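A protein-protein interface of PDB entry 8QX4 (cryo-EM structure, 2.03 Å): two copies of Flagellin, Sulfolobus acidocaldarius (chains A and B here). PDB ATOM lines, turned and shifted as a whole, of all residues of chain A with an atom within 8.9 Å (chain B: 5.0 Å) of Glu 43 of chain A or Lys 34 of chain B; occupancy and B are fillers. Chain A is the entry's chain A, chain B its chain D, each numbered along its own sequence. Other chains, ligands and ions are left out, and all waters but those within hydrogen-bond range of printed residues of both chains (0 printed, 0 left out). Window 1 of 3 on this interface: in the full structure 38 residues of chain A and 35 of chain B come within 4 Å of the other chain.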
ATOM      1  N   LYS A  36      -8.217  -8.802 -16.190  1.00  0.00           N
ATOM      2  CA  LYS A  36      -9.022  -9.349 -17.281  1.00  0.00           C
ATOM      3  C   LYS A  36     -10.364  -8.617 -17.404  1.00  0.00           C
ATOM      4  O   LYS A  36     -10.721  -8.147 -18.489  1.00  0.00           O
ATOM      5  CB  LYS A  36      -9.206 -10.861 -17.107  1.00  0.00           C
ATOM      6  CG  LYS A  36      -9.969 -11.554 -18.227  1.00  0.00           C
ATOM      7  CD  LYS A  36     -10.113 -13.051 -18.034  1.00  0.00           C
ATOM      8  CE  LYS A  36     -10.693 -13.768 -19.238  1.00  0.00           C
ATOM      9  NZ  LYS A  36     -12.132 -13.465 -19.429  1.00  0.00           N
ATOM     10  N   THR A  37     -11.089  -8.507 -16.281  1.00  0.00           N
ATOM     11  CA  THR A  37     -12.382  -7.838 -16.199  1.00  0.00           C
ATOM     12  C   THR A  37     -12.269  -6.378 -16.644  1.00  0.00           C
ATOM     13  O   THR A  37     -13.089  -5.914 -17.433  1.00  0.00           O
ATOM     14  CB  THR A  37     -12.990  -7.965 -14.794  1.00  0.00           C
ATOM     15  OG1 THR A  37     -13.073  -9.347 -14.441  1.00  0.00           O
ATOM     16  CG2 THR A  37     -14.358  -7.328 -14.672  1.00  0.00           C
ATOM     17  N   THR A  38     -11.238  -5.671 -16.158  1.00  0.00           N
ATOM     18  CA  THR A  38     -10.973  -4.276 -16.493  1.00  0.00           C
ATOM     19  C   THR A  38     -10.737  -4.100 -17.995  1.00  0.00           C
ATOM     20  O   THR A  38     -11.300  -3.188 -18.592  1.00  0.00           O
ATOM     21  CB  THR A  38      -9.809  -3.706 -15.671  1.00  0.00           C
ATOM     22  OG1 THR A  38     -10.189  -3.733 -14.295  1.00  0.00           O
ATOM     23  CG2 THR A  38      -9.421  -2.294 -16.051  1.00  0.00           C
ATOM     24  N   ILE A  39      -9.913  -4.966 -18.601  1.00  0.00           N
ATOM     25  CA  ILE A  39      -9.609  -4.909 -20.027  1.00  0.00           C
ATOM     26  C   ILE A  39     -10.892  -5.059 -20.853  1.00  0.00           C
ATOM     27  O   ILE A  39     -11.101  -4.306 -21.803  1.00  0.00           O
ATOM     28  CB  ILE A  39      -8.508  -5.921 -20.415  1.00  0.00           C
ATOM     29  CG1 ILE A  39      -7.183  -5.627 -19.701  1.00  0.00           C
ATOM     30  CG2 ILE A  39      -8.314  -5.939 -21.923  1.00  0.00           C
ATOM     31  CD1 ILE A  39      -6.283  -6.835 -19.527  1.00  0.00           C
ATOM     32  N   ASN A  40     -11.767  -5.994 -20.464  1.00  0.00           N
ATOM     33  CA  ASN A  40     -13.067  -6.173 -21.094  1.00  0.00           C
ATOM     34  C   ASN A  40     -13.929  -4.908 -20.983  1.00  0.00           C
ATOM     35  O   ASN A  40     -14.455  -4.428 -21.989  1.00  0.00           O
ATOM     36  CB  ASN A  40     -13.770  -7.419 -20.564  1.00  0.00           C
ATOM     37  CG  ASN A  40     -15.078  -7.645 -21.284  1.00  0.00           C
ATOM     38  OD1 ASN A  40     -15.090  -7.886 -22.489  1.00  0.00           O
ATOM     39  ND2 ASN A  40     -16.183  -7.510 -20.570  1.00  0.00           N
ATOM     40  N   LYS A  41     -14.038  -4.332 -19.776  1.00  0.00           N
ATOM     41  CA  LYS A  41     -14.804  -3.110 -19.537  1.00  0.00           C
ATOM     42  C   LYS A  41     -14.247  -1.907 -20.307  1.00  0.00           C
ATOM     43  O   LYS A  41     -15.016  -1.061 -20.751  1.00  0.00           O
ATOM     44  CB  LYS A  41     -14.934  -2.818 -18.038  1.00  0.00           C
ATOM     45  CG  LYS A  41     -15.870  -3.743 -17.271  1.00  0.00           C
ATOM     46  CD  LYS A  41     -17.332  -3.569 -17.631  1.00  0.00           C
ATOM     47  CE  LYS A  41     -18.169  -4.799 -17.355  1.00  0.00           C
ATOM     48  NZ  LYS A  41     -19.441  -4.771 -18.117  1.00  0.00           N
ATOM     49  N   GLY A  42     -12.921  -1.833 -20.477  1.00  0.00           N
ATOM     50  CA  GLY A  42     -12.275  -0.812 -21.292  1.00  0.00           C
ATOM     51  C   GLY A  42     -12.670  -0.902 -22.768  1.00  0.00           C
ATOM     52  O   GLY A  42     -12.991   0.114 -23.381  1.00  0.00           O
ATOM     53  N   GLU A  43     -12.689  -2.124 -23.318  1.00  0.00           N
ATOM     54  CA  GLU A  43     -13.093  -2.366 -24.698  1.00  0.00           C
ATOM     55  C   GLU A  43     -14.587  -2.071 -24.898  1.00  0.00           C
ATOM     56  O   GLU A  43     -14.963  -1.435 -25.881  1.00  0.00           O
ATOM     57  CB  GLU A  43     -12.662  -3.769 -25.136  1.00  0.00           C
ATOM     58  CG  GLU A  43     -12.907  -4.062 -26.611  1.00  0.00           C
ATOM     59  CD  GLU A  43     -14.326  -4.436 -27.018  1.00  0.00           C
ATOM     60  OE1 GLU A  43     -15.006  -5.134 -26.235  1.00  0.00           O
ATOM     61  OE2 GLU A  43     -14.747  -4.042 -28.129  1.00  0.00           O
ATOM     62  N   GLU A  44     -15.438  -2.502 -23.957  1.00  0.00           N
ATOM     63  CA  GLU A  44     -16.858  -2.162 -23.959  1.00  0.00           C
ATOM     64  C   GLU A  44     -17.065  -0.644 -23.949  1.00  0.00           C
ATOM     65  O   GLU A  44     -17.874  -0.137 -24.719  1.00  0.00           O
ATOM     66  CB  GLU A  44     -17.581  -2.831 -22.789  1.00  0.00           C
ATOM     67  CG  GLU A  44     -17.756  -4.329 -22.958  1.00  0.00           C
ATOM     68  CD  GLU A  44     -18.351  -5.074 -21.772  1.00  0.00           C
ATOM     69  OE1 GLU A  44     -18.742  -4.419 -20.781  1.00  0.00           O
ATOM     70  OE2 GLU A  44     -18.433  -6.318 -21.846  1.00  0.00           O
ATOM     71  N   THR A  45     -16.302   0.081 -23.119  1.00  0.00           N
ATOM     72  CA  THR A  45     -16.382   1.534 -22.997  1.00  0.00           C
ATOM     73  C   THR A  45     -15.974   2.238 -24.294  1.00  0.00           C
ATOM     74  O   THR A  45     -16.596   3.223 -24.678  1.00  0.00           O
ATOM     75  CB  THR A  45     -15.566   2.031 -21.793  1.00  0.00           C
ATOM     76  OG1 THR A  45     -16.187   1.491 -20.627  1.00  0.00           O
ATOM     77  CG2 THR A  45     -15.492   3.538 -21.677  1.00  0.00           C
ATOM     78  N   ALA A  46     -14.924   1.751 -24.964  1.00  0.00           N
ATOM     79  CA  ALA A  46     -14.449   2.343 -26.208  1.00  0.00           C
ATOM     80  C   ALA A  46     -15.386   2.052 -27.386  1.00  0.00           C
ATOM     81  O   ALA A  46     -15.528   2.891 -28.275  1.00  0.00           O
ATOM     82  CB  ALA A  46     -13.040   1.884 -26.486  1.00  0.00           C
ATOM     83  N   SER A  47     -16.020   0.867 -27.396  1.00  0.00           N
ATOM     84  CA  SER A  47     -16.870   0.419 -28.495  1.00  0.00           C
ATOM     85  C   SER A  47     -18.294   0.982 -28.417  1.00  0.00           C
ATOM     86  O   SER A  47     -18.817   1.460 -29.422  1.00  0.00           O
ATOM     87  CB  SER A  47     -16.856  -1.087 -28.630  1.00  0.00           C
ATOM     88  OG  SER A  47     -17.303  -1.708 -27.435  1.00  0.00           O
ATOM     89  N   THR A  48     -18.929   0.928 -27.236  1.00  0.00           N
ATOM     90  CA  THR A  48     -20.345   1.269 -27.095  1.00  0.00           C
ATOM     91  C   THR A  48     -20.598   2.776 -27.229  1.00  0.00           C
ATOM     92  O   THR A  48     -20.025   3.581 -26.493  1.00  0.00           O
ATOM     93  CB  THR A  48     -20.955   0.692 -25.807  1.00  0.00           C
ATOM     94  OG1 THR A  48     -20.184   1.105 -24.681  1.00  0.00           O
ATOM     95  CG2 THR A  48     -20.997  -0.819 -25.784  1.00  0.00           C
ATOM     96  N   ALA A  49     -21.503   3.147 -28.153  1.00  0.00           N
ATOM     97  CA  ALA A  49     -21.906   4.530 -28.386  1.00  0.00           C
ATOM     98  C   ALA A  49     -23.219   4.586 -29.170  1.00  0.00           C
ATOM     99  O   ALA A  49     -23.543   3.647 -29.894  1.00  0.00           O
ATOM    100  CB  ALA A  49     -20.815   5.271 -29.124  1.00  0.00           C
ATOM    101  N   VAL A  81     -21.123  -1.566 -34.047  1.00  0.00           N
ATOM    102  CA  VAL A  81     -20.024  -2.279 -33.396  1.00  0.00           C
ATOM    103  C   VAL A  81     -20.485  -3.146 -32.215  1.00  0.00           C
ATOM    104  O   VAL A  81     -19.975  -4.257 -32.046  1.00  0.00           O
ATOM    105  CB  VAL A  81     -18.811  -1.384 -33.055  1.00  0.00           C
ATOM    106  CG1 VAL A  81     -18.228  -0.733 -34.298  1.00  0.00           C
ATOM    107  CG2 VAL A  81     -19.134  -0.321 -32.017  1.00  0.00           C
ATOM    108  N   SER A  82     -21.407  -2.632 -31.379  1.00  0.00           N
ATOM    109  CA  SER A  82     -21.884  -3.326 -30.183  1.00  0.00           C
ATOM    110  C   SER A  82     -23.225  -2.768 -29.691  1.00  0.00           C
ATOM    111  O   SER A  82     -23.621  -1.680 -30.093  1.00  0.00           O
ATOM    112  CB  SER A  82     -20.832  -3.347 -29.081  1.00  0.00           C
ATOM    113  OG  SER A  82     -20.361  -2.040 -28.767  1.00  0.00           O
ATOM    114  N   SER A  83     -23.909  -3.516 -28.808  1.00  0.00           N
ATOM    115  CA  SER A  83     -25.229  -3.174 -28.276  1.00  0.00           C
ATOM    116  C   SER A  83     -25.163  -2.115 -27.168  1.00  0.00           C
ATOM    117  O   SER A  83     -24.131  -1.949 -26.524  1.00  0.00           O
ATOM    118  CB  SER A  83     -25.933  -4.411 -27.783  1.00  0.00           C
ATOM    119  OG  SER A  83     -25.187  -5.029 -26.745  1.00  0.00           O
ATOM    120  N   ILE A 272     -22.855   2.190 -19.689  1.00  0.00           N
ATOM    121  CA  ILE A 272     -21.575   1.800 -20.273  1.00  0.00           C
ATOM    122  C   ILE A 272     -21.414   2.586 -21.573  1.00  0.00           C
ATOM    123  O   ILE A 272     -22.382   2.773 -22.304  1.00  0.00           O
ATOM    124  CB  ILE A 272     -21.502   0.270 -20.513  1.00  0.00           C
ATOM    125  CG1 ILE A 272     -21.723  -0.549 -19.234  1.00  0.00           C
ATOM    126  CG2 ILE A 272     -20.197  -0.121 -21.196  1.00  0.00           C
ATOM    127  CD1 ILE A 272     -22.099  -2.002 -19.468  1.00  0.00           C
ATOM    128  N   GLY A 273     -20.190   3.049 -21.855  1.00  0.00           N
ATOM    129  CA  GLY A 273     -19.894   3.722 -23.110  1.00  0.00           C
ATOM    130  C   GLY A 273     -20.103   5.233 -23.049  1.00  0.00           C
ATOM    131  O   GLY A 273     -20.576   5.775 -22.050  1.00  0.00           O
ATOM    132  N   PHE B  30      -7.913 -11.656 -27.506  1.00  0.00           N
ATOM    133  CA  PHE B  30      -9.306 -11.238 -27.488  1.00  0.00           C
ATOM    134  C   PHE B  30      -9.475  -9.801 -27.999  1.00  0.00           C
ATOM    135  O   PHE B  30     -10.172  -9.581 -28.990  1.00  0.00           O
ATOM    136  CB  PHE B  30      -9.898 -11.463 -26.095  1.00  0.00           C
ATOM    137  CG  PHE B  30     -11.351 -11.080 -25.976  1.00  0.00           C
ATOM    138  CD1 PHE B  30     -12.354 -11.998 -26.263  1.00  0.00           C
ATOM    139  CD2 PHE B  30     -11.723  -9.798 -25.591  1.00  0.00           C
ATOM    140  CE1 PHE B  30     -13.692 -11.647 -26.159  1.00  0.00           C
ATOM    141  CE2 PHE B  30     -13.064  -9.443 -25.493  1.00  0.00           C
ATOM    142  CZ  PHE B  30     -14.045 -10.370 -25.775  1.00  0.00           C
ATOM    143  N   VAL B  31      -8.827  -8.828 -27.342  1.00  0.00           N
ATOM    144  CA  VAL B  31      -9.015  -7.407 -27.630  1.00  0.00           C
ATOM    145  C   VAL B  31      -8.576  -7.056 -29.055  1.00  0.00           C
ATOM    146  O   VAL B  31      -9.266  -6.299 -29.735  1.00  0.00           O
ATOM    147  CB  VAL B  31      -8.355  -6.506 -26.567  1.00  0.00           C
ATOM    148  CG1 VAL B  31      -8.304  -5.040 -26.977  1.00  0.00           C
ATOM    149  CG2 VAL B  31      -9.063  -6.639 -25.233  1.00  0.00           C
ATOM    150  N   THR B  32      -7.453  -7.619 -29.522  1.00  0.00           N
ATOM    151  CA  THR B  32      -6.973  -7.355 -30.874  1.00  0.00           C
ATOM    152  C   THR B  32      -7.956  -7.858 -31.930  1.00  0.00           C
ATOM    153  O   THR B  32      -8.123  -7.210 -32.957  1.00  0.00           O
ATOM    154  CB  THR B  32      -5.544  -7.858 -31.111  1.00  0.00           C
ATOM    155  OG1 THR B  32      -5.507  -9.259 -30.844  1.00  0.00           O
ATOM    156  CG2 THR B  32      -4.524  -7.136 -30.261  1.00  0.00           C
ATOM    157  N   GLN B  33      -8.666  -8.957 -31.663  1.00  0.00           N
ATOM    158  CA  GLN B  33      -9.712  -9.428 -32.562  1.00  0.00           C
ATOM    159  C   GLN B  33     -10.945  -8.510 -32.551  1.00  0.00           C
ATOM    160  O   GLN B  33     -11.546  -8.281 -33.605  1.00  0.00           O
ATOM    161  CB  GLN B  33     -10.042 -10.874 -32.221  1.00  0.00           C
ATOM    162  CG  GLN B  33     -10.867 -11.555 -33.300  1.00  0.00           C
ATOM    163  CD  GLN B  33     -11.357 -12.923 -32.892  1.00  0.00           C
ATOM    164  OE1 GLN B  33     -12.556 -13.194 -32.885  1.00  0.00           O
ATOM    165  NE2 GLN B  33     -10.430 -13.806 -32.551  1.00  0.00           N
ATOM    166  N   LYS B  34     -11.322  -7.975 -31.378  1.00  0.00           N
ATOM    167  CA  LYS B  34     -12.366  -6.958 -31.275  1.00  0.00           C
ATOM    168  C   LYS B  34     -12.000  -5.724 -32.107  1.00  0.00           C
ATOM    169  O   LYS B  34     -12.845  -5.191 -32.825  1.00  0.00           O
ATOM    170  CB  LYS B  34     -12.662  -6.594 -29.813  1.00  0.00           C
ATOM    171  CG  LYS B  34     -13.131  -7.728 -28.906  1.00  0.00           C
ATOM    172  CD  LYS B  34     -14.521  -8.274 -29.200  1.00  0.00           C
ATOM    173  CE  LYS B  34     -15.644  -7.312 -28.867  1.00  0.00           C
ATOM    174  NZ  LYS B  34     -16.976  -7.907 -29.132  1.00  0.00           N
ATOM    175  N   ALA B  35     -10.727  -5.303 -32.046  1.00  0.00           N
ATOM    176  CA  ALA B  35     -10.191  -4.226 -32.870  1.00  0.00           C
ATOM    177  C   ALA B  35     -10.306  -4.547 -34.365  1.00  0.00           C
ATOM    178  O   ALA B  35     -10.826  -3.721 -35.110  1.00  0.00           O
ATOM    179  CB  ALA B  35      -8.784  -3.871 -32.444  1.00  0.00           C
ATOM    180  N   LYS B  36      -9.883  -5.747 -34.803  1.00  0.00           N
ATOM    181  CA  LYS B  36     -10.017  -6.198 -36.187  1.00  0.00           C
ATOM    182  C   LYS B  36     -11.464  -6.068 -36.677  1.00  0.00           C
ATOM    183  O   LYS B  36     -11.715  -5.467 -37.725  1.00  0.00           O
ATOM    184  CB  LYS B  36      -9.485  -7.629 -36.340  1.00  0.00           C
ATOM    185  CG  LYS B  36      -9.503  -8.173 -37.761  1.00  0.00           C
ATOM    186  CD  LYS B  36      -8.945  -9.578 -37.887  1.00  0.00           C
ATOM    187  CE  LYS B  36      -8.778 -10.041 -39.322  1.00  0.00           C
ATOM    188  NZ  LYS B  36     -10.081 -10.272 -39.991  1.00  0.00           N
ATOM    189  N   THR B  37     -12.409  -6.616 -35.900  1.00  0.00           N
ATOM    190  CA  THR B  37     -13.837  -6.584 -36.195  1.00  0.00           C
ATOM    191  C   THR B  37     -14.333  -5.143 -36.324  1.00  0.00           C
ATOM    192  O   THR B  37     -15.046  -4.824 -37.275  1.00  0.00           O
ATOM    193  CB  THR B  37     -14.642  -7.377 -35.154  1.00  0.00           C
ATOM    194  OG1 THR B  37     -14.135  -8.710 -35.082  1.00  0.00           O
ATOM    195  CG2 THR B  37     -16.126  -7.417 -35.449  1.00  0.00           C
ATOM    196  N   THR B  38     -13.934  -4.273 -35.384  1.00  0.00           N
ATOM    197  CA  THR B  38     -14.300  -2.860 -35.368  1.00  0.00           C
ATOM    198  C   THR B  38     -13.806  -2.145 -36.627  1.00  0.00           C
ATOM    199  O   THR B  38     -14.568  -1.397 -37.233  1.00  0.00           O
ATOM    200  CB  THR B  38     -13.808  -2.162 -34.094  1.00  0.00           C
ATOM    201  OG1 THR B  38     -14.461  -2.769 -32.979  1.00  0.00           O
ATOM    202  CG2 THR B  38     -14.072  -0.671 -34.074  1.00  0.00           C
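The side-chain amide nitrogen of Asn 40 of chain A sits at hydrogen-bond distance from the side-chain carboxylate of Glu 44 of chain A (2.8 Å).
OG of Ser 47 of chain A is in hydrogen-bond range of O of Glu 43 of chain A (2.8 Å).
O of Lys 34 of chain B is in hydrogen-bond range of OG1 of Thr 38 of chain B (2.9 Å).
Ile 39 of chain A touches Val 31 of chain B (CG2 to CG2, 3.5 Å).
CE2 of Phe 30 of chain B touches OD1 of Asn 40 of chain A, 3.9 Å away.
Glu 43 of chain A touches Lys 34 of chain B (OE2 to CE, 3.5 Å).
Of the printed residues of chain B, Ile 39 of chain A touches Val 31.
Of chain B, only Lys 34 (3.5 Å) comes within 4 Å of Glu 43 of chain A.
Ser 83 of chain A touches none of the printed residues of chain B.
Of the printed residues of chain A, Val 31 of chain B touches Ile 39 (3.5 Å).
No residue of chain A comes within 4 Å of Ala 35 of chain B.
Thr 37 of chain B touches none of the printed residues of chain A.
Of the 19 printed residues of chain A, 3 touch a printed residue of chain B.
Hydrophobic or aromatic side chains of chain A that line the printed part of chain B: Ile 39.
Printed residues of chain B that touch a printed residue of chain A: Phe 30, Val 31 and Lys 34.
Hydrophobic or aromatic side chains of chain B within 4 Å of the printed part of chain A: Phe 30 and Val 31.
3 positions are printed for both chains.
Of the 3 pairs that touch across the chains among the printed residues, none has its exchanged pair printed and touching as well.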
